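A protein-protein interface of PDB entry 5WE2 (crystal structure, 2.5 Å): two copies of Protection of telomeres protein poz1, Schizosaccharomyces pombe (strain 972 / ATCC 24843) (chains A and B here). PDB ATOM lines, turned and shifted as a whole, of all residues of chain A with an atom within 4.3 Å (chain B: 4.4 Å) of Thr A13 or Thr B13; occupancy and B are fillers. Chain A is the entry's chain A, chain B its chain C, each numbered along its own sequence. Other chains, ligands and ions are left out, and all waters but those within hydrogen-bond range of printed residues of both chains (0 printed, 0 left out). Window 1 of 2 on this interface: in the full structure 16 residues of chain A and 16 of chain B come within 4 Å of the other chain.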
ATOM      1  N   SER A   9      12.955 -10.315  21.769  1.00  0.00           N
ATOM      2  CA  SER A   9      12.895  -9.063  22.494  1.00  0.00           C
ATOM      3  C   SER A   9      13.221  -7.891  21.544  1.00  0.00           C
ATOM      4  O   SER A   9      12.581  -6.830  21.611  1.00  0.00           O
ATOM      5  CB  SER A   9      13.832  -9.114  23.697  1.00  0.00           C
ATOM      6  OG  SER A   9      13.629  -7.991  24.522  1.00  0.00           O
ATOM      7  N   VAL A  10      14.181  -8.102  20.636  1.00  0.00           N
ATOM      8  CA  VAL A  10      14.589  -7.060  19.675  1.00  0.00           C
ATOM      9  C   VAL A  10      13.439  -6.736  18.683  1.00  0.00           C
ATOM     10  O   VAL A  10      13.220  -5.580  18.297  1.00  0.00           O
ATOM     11  CB  VAL A  10      15.869  -7.494  18.903  1.00  0.00           C
ATOM     12  CG1 VAL A  10      16.175  -6.567  17.725  1.00  0.00           C
ATOM     13  CG2 VAL A  10      17.043  -7.567  19.852  1.00  0.00           C
ATOM     14  N   LEU A  11      12.703  -7.770  18.289  1.00  0.00           N
ATOM     15  CA  LEU A  11      11.484  -7.585  17.511  1.00  0.00           C
ATOM     16  C   LEU A  11      10.476  -6.718  18.262  1.00  0.00           C
ATOM     17  O   LEU A  11       9.957  -5.736  17.687  1.00  0.00           O
ATOM     18  CB  LEU A  11      10.864  -8.932  17.159  1.00  0.00           C
ATOM     19  CG  LEU A  11      11.506  -9.591  15.942  1.00  0.00           C
ATOM     20  CD1 LEU A  11      10.795 -10.881  15.578  1.00  0.00           C
ATOM     21  CD2 LEU A  11      11.495  -8.608  14.775  1.00  0.00           C
ATOM     22  N   ASN A  12      10.210  -7.061  19.536  1.00  0.00           N
ATOM     23  CA  ASN A  12       9.286  -6.257  20.354  1.00  0.00           C
ATOM     24  C   ASN A  12       9.740  -4.807  20.376  1.00  0.00           C
ATOM     25  O   ASN A  12       8.919  -3.901  20.418  1.00  0.00           O
ATOM     26  CB  ASN A  12       9.171  -6.742  21.813  1.00  0.00           C
ATOM     27  CG  ASN A  12       8.660  -8.165  21.942  1.00  0.00           C
ATOM     28  OD1 ASN A  12       8.070  -8.729  21.018  1.00  0.00           O
ATOM     29  ND2 ASN A  12       8.905  -8.765  23.108  1.00  0.00           N
ATOM     30  N   THR A  13      11.046  -4.574  20.385  1.00  0.00           N
ATOM     31  CA  THR A  13      11.507  -3.186  20.397  1.00  0.00           C
ATOM     32  C   THR A  13      11.246  -2.540  19.045  1.00  0.00           C
ATOM     33  O   THR A  13      10.922  -1.351  18.966  1.00  0.00           O
ATOM     34  CB  THR A  13      13.003  -3.079  20.776  1.00  0.00           C
ATOM     35  OG1 THR A  13      13.138  -3.296  22.185  1.00  0.00           O
ATOM     36  CG2 THR A  13      13.549  -1.711  20.470  1.00  0.00           C
ATOM     37  N   LEU A  14      11.358  -3.320  17.977  1.00  0.00           N
ATOM     38  CA  LEU A  14      11.128  -2.748  16.655  1.00  0.00           C
ATOM     39  C   LEU A  14       9.671  -2.373  16.425  1.00  0.00           C
ATOM     40  O   LEU A  14       9.409  -1.321  15.844  1.00  0.00           O
ATOM     41  CB  LEU A  14      11.612  -3.696  15.561  1.00  0.00           C
ATOM     42  CG  LEU A  14      13.090  -3.417  15.301  1.00  0.00           C
ATOM     43  CD1 LEU A  14      13.636  -4.348  14.267  1.00  0.00           C
ATOM     44  CD2 LEU A  14      13.329  -1.955  14.922  1.00  0.00           C
ATOM     45  N   GLU A  15       8.731  -3.205  16.881  1.00  0.00           N
ATOM     46  CA  GLU A  15       7.303  -2.837  16.864  1.00  0.00           C
ATOM     47  C   GLU A  15       7.103  -1.386  17.266  1.00  0.00           C
ATOM     48  O   GLU A  15       6.486  -0.606  16.549  1.00  0.00           O
ATOM     49  CB  GLU A  15       6.488  -3.724  17.804  1.00  0.00           C
ATOM     50  CG  GLU A  15       6.207  -5.108  17.263  1.00  0.00           C
ATOM     51  CD  GLU A  15       5.166  -5.841  18.095  1.00  0.00           C
ATOM     52  OE1 GLU A  15       4.913  -5.396  19.234  1.00  0.00           O
ATOM     53  OE2 GLU A  15       4.595  -6.849  17.613  1.00  0.00           O
ATOM     54  N   THR A  16       7.683  -1.030  18.401  1.00  0.00           N
ATOM     55  CA  THR A  16       7.570   0.304  18.983  1.00  0.00           C
ATOM     56  C   THR A  16       8.213   1.405  18.114  1.00  0.00           C
ATOM     57  O   THR A  16       8.163   2.605  18.434  1.00  0.00           O
ATOM     58  CB  THR A  16       8.211   0.270  20.407  1.00  0.00           C
ATOM     59  OG1 THR A  16       7.732  -0.885  21.124  1.00  0.00           O
ATOM     60  CG2 THR A  16       7.851   1.475  21.195  1.00  0.00           C
ATOM     61  N   PHE A  17       8.818   1.006  17.003  1.00  0.00           N
ATOM     62  CA  PHE A  17       9.480   1.966  16.129  1.00  0.00           C
ATOM     63  C   PHE A  17       8.834   1.955  14.760  1.00  0.00           C
ATOM     64  O   PHE A  17       8.907   2.934  14.029  1.00  0.00           O
ATOM     65  CB  PHE A  17      10.999   1.645  16.004  1.00  0.00           C
ATOM     66  CG  PHE A  17      11.827   2.293  17.063  1.00  0.00           C
ATOM     67  CD1 PHE A  17      12.286   3.596  16.901  1.00  0.00           C
ATOM     68  CD2 PHE A  17      12.082   1.641  18.249  1.00  0.00           C
ATOM     69  CE1 PHE A  17      13.014   4.216  17.894  1.00  0.00           C
ATOM     70  CE2 PHE A  17      12.808   2.259  19.245  1.00  0.00           C
ATOM     71  CZ  PHE A  17      13.273   3.542  19.070  1.00  0.00           C
ATOM     72  N   SER B   9      10.509  -0.319  26.052  1.00  0.00           N
ATOM     73  CA  SER B   9      10.848  -1.469  25.224  1.00  0.00           C
ATOM     74  C   SER B   9      12.387  -1.716  25.153  1.00  0.00           C
ATOM     75  O   SER B   9      12.877  -2.851  25.273  1.00  0.00           O
ATOM     76  CB  SER B   9      10.295  -1.275  23.833  1.00  0.00           C
ATOM     77  OG  SER B   9      10.167  -2.531  23.215  1.00  0.00           O
ATOM     78  N   VAL B  10      13.126  -0.636  24.940  1.00  0.00           N
ATOM     79  CA  VAL B  10      14.557  -0.698  24.843  1.00  0.00           C
ATOM     80  C   VAL B  10      15.088  -1.239  26.173  1.00  0.00           C
ATOM     81  O   VAL B  10      15.880  -2.183  26.201  1.00  0.00           O
ATOM     82  CB  VAL B  10      15.128   0.681  24.492  1.00  0.00           C
ATOM     83  CG1 VAL B  10      16.626   0.660  24.539  1.00  0.00           C
ATOM     84  CG2 VAL B  10      14.659   1.076  23.109  1.00  0.00           C
ATOM     85  N   LEU B  11      14.575  -0.710  27.279  1.00  0.00           N
ATOM     86  CA  LEU B  11      14.958  -1.252  28.577  1.00  0.00           C
ATOM     87  C   LEU B  11      14.648  -2.760  28.699  1.00  0.00           C
ATOM     88  O   LEU B  11      15.482  -3.523  29.226  1.00  0.00           O
ATOM     89  CB  LEU B  11      14.290  -0.451  29.690  1.00  0.00           C
ATOM     90  CG  LEU B  11      14.691  -0.679  31.143  1.00  0.00           C
ATOM     91  CD1 LEU B  11      16.158  -0.339  31.394  1.00  0.00           C
ATOM     92  CD2 LEU B  11      13.781   0.138  32.046  1.00  0.00           C
ATOM     93  N   ASN B  12      13.500  -3.222  28.189  1.00  0.00           N
ATOM     94  CA  ASN B  12      13.215  -4.676  28.246  1.00  0.00           C
ATOM     95  C   ASN B  12      14.195  -5.545  27.437  1.00  0.00           C
ATOM     96  O   ASN B  12      14.566  -6.678  27.830  1.00  0.00           O
ATOM     97  CB  ASN B  12      11.799  -4.966  27.761  1.00  0.00           C
ATOM     98  CG  ASN B  12      10.728  -4.339  28.644  1.00  0.00           C
ATOM     99  OD1 ASN B  12      10.934  -4.094  29.835  1.00  0.00           O
ATOM    100  ND2 ASN B  12       9.574  -4.078  28.054  1.00  0.00           N
ATOM    101  N   THR B  13      14.594  -5.020  26.285  1.00  0.00           N
ATOM    102  CA  THR B  13      15.594  -5.703  25.481  1.00  0.00           C
ATOM    103  C   THR B  13      16.941  -5.793  26.214  1.00  0.00           C
ATOM    104  O   THR B  13      17.522  -6.897  26.358  1.00  0.00           O
ATOM    105  CB  THR B  13      15.761  -5.009  24.137  1.00  0.00           C
ATOM    106  OG1 THR B  13      14.510  -5.092  23.426  1.00  0.00           O
ATOM    107  CG2 THR B  13      16.896  -5.671  23.329  1.00  0.00           C
ATOM    108  N   LEU B  14      17.422  -4.651  26.703  1.00  0.00           N
ATOM    109  CA  LEU B  14      18.593  -4.666  27.592  1.00  0.00           C
ATOM    110  C   LEU B  14      18.473  -5.713  28.702  1.00  0.00           C
ATOM    111  O   LEU B  14      19.422  -6.447  28.959  1.00  0.00           O
ATOM    112  CB  LEU B  14      18.836  -3.296  28.211  1.00  0.00           C
ATOM    113  CG  LEU B  14      19.772  -2.432  27.367  1.00  0.00           C
ATOM    114  CD1 LEU B  14      19.988  -1.063  27.988  1.00  0.00           C
ATOM    115  CD2 LEU B  14      21.116  -3.132  27.125  1.00  0.00           C
ATOM    116  N   GLU B  15      17.317  -5.810  29.345  1.00  0.00           N
ATOM    117  CA  GLU B  15      17.144  -6.832  30.379  1.00  0.00           C
ATOM    118  C   GLU B  15      17.412  -8.209  29.818  1.00  0.00           C
ATOM    119  O   GLU B  15      18.072  -9.046  30.452  1.00  0.00           O
ATOM    120  CB  GLU B  15      15.744  -6.786  30.984  1.00  0.00           C
ATOM    121  CG  GLU B  15      15.444  -7.964  31.878  1.00  0.00           C
ATOM    122  CD  GLU B  15      14.180  -7.790  32.697  1.00  0.00           C
ATOM    123  OE1 GLU B  15      13.733  -8.789  33.315  1.00  0.00           O
ATOM    124  OE2 GLU B  15      13.641  -6.658  32.725  1.00  0.00           O
ATOM    125  N   THR B  16      16.921  -8.447  28.614  1.00  0.00           N
ATOM    126  CA  THR B  16      17.206  -9.721  27.959  1.00  0.00           C
ATOM    127  C   THR B  16      18.712  -9.955  27.681  1.00  0.00           C
ATOM    128  O   THR B  16      19.182 -11.091  27.669  1.00  0.00           O
ATOM    129  CB  THR B  16      16.394  -9.813  26.655  1.00  0.00           C
ATOM    130  OG1 THR B  16      15.018  -9.572  26.976  1.00  0.00           O
ATOM    131  CG2 THR B  16      16.462 -11.166  26.110  1.00  0.00           C
ATOM    132  N   PHE B  17      19.477  -8.893  27.447  1.00  0.00           N
ATOM    133  CA  PHE B  17      20.900  -9.079  27.167  1.00  0.00           C
ATOM    134  C   PHE B  17      21.764  -9.104  28.440  1.00  0.00           C
ATOM    135  O   PHE B  17      22.871  -9.637  28.435  1.00  0.00           O
ATOM    136  CB  PHE B  17      21.425  -7.972  26.239  1.00  0.00           C
ATOM    137  CG  PHE B  17      21.051  -8.150  24.792  1.00  0.00           C
ATOM    138  CD1 PHE B  17      19.736  -7.965  24.358  1.00  0.00           C
ATOM    139  CD2 PHE B  17      22.024  -8.461  23.851  1.00  0.00           C
ATOM    140  CE1 PHE B  17      19.404  -8.118  23.024  1.00  0.00           C
ATOM    141  CE2 PHE B  17      21.696  -8.610  22.506  1.00  0.00           C
ATOM    142  CZ  PHE B  17      20.369  -8.434  22.094  1.00  0.00           C
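The backbone carbonyl oxygen (O) of Ser A9 sits at hydrogen-bond distance from the side-chain hydroxyl (OG1) of Thr B13, at 3.2 Å. OG of Ser A9 sits at hydrogen-bond distance from OG1 of Thr B16, 3.2 Å away. The backbone carbonyl oxygen of Asn A12 is in hydrogen-bond range of the side-chain hydroxyl of Ser B9, at 3.4 Å. OG1 of Thr A13 lies within hydrogen-bond range of O of Ser B9, at 3.1 Å. The side-chain hydroxyl of Thr B13 sits at hydrogen-bond distance from the side-chain hydroxyl of Thr A13 (2.6 Å).
The backbone carbonyl oxygen (O) of Asn A12 is in hydrogen-bond range of the side-chain hydroxyl (OG1) of Thr A16 (3.3 Å). OG1 of Thr B13 lies within hydrogen-bond range of O of Ser B9, at 3.3 Å. The backbone carbonyl oxygen (O) of Asn B12 is in hydrogen-bond range of the side-chain hydroxyl (OG1) of Thr B16, at 3.1 Å.
Ser A9 touches Asn B12 (OG to O, 3.7 Å). Thr B13 touches Val A10 (CG2 to CG2, 3.96 Å). Val A10 touches Phe B17 (CG2 to CE1, 3.99 Å). Val B10 touches Thr A13 (N to OG1, 3.8 Å). OG1 of Thr A16 touches OG of Ser B9, at 3.6 Å.
Of chain A, only Ser A9, Val A10 and Thr A13 come within 4 Å of Thr B13. Printed residues of chain B within 4 Å of Val A10: Thr B13 and Phe B17. Of the printed residues of chain B, Asn A12 touches Ser B9. Printed residues of chain A within 4 Å of Ser B9: Asn A12, Thr A13 and Thr A16. Of the printed residues of chain A, Val B10 touches Thr A13 (3.8 Å). Printed residues of chain B within 4 Å of Ser A9: Asn B12 (3.7 Å), Thr B13 (3.2 Å) and Thr B16 (3.2 Å). Leu B14 touches none of the printed residues of chain A. The nearest printed residue of chain A that does not touch Thr B13 is Asn A12 (5.7 Å).
Of the 9 printed residues of chain A, 5 touch a printed residue of chain B. Of the 9 printed residues of chain B, 6 touch a printed residue of chain A. Printed residues of chain B that touch a printed residue of chain A: Ser B9, Val B10, Asn B12, Thr B13, Thr B16 and Phe B17. Hydrophobic or aromatic side chains of chain B within 4 Å of the printed part of chain A: Val B10 and Phe B17. Among the printed residues, no Asp or Glu carboxylate lies within 4 Å of a Lys or Arg side-chain nitrogen of the other chain.
Ser A9 touches Asn B12, and with the chains exchanged Asn A12 touches Ser B9. Ser A9 touches Thr B13, and with the chains exchanged Thr A13 touches Ser B9. Ser A9 touches Thr B16, and with the chains exchanged Thr A16 touches Ser B9. Val A10 touches Thr B13, and with the chains exchanged Thr A13 touches Val B10. Of the 10 pairs that touch across the chains among the printed residues, 9 have their exchanged pair printed and touching as well.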
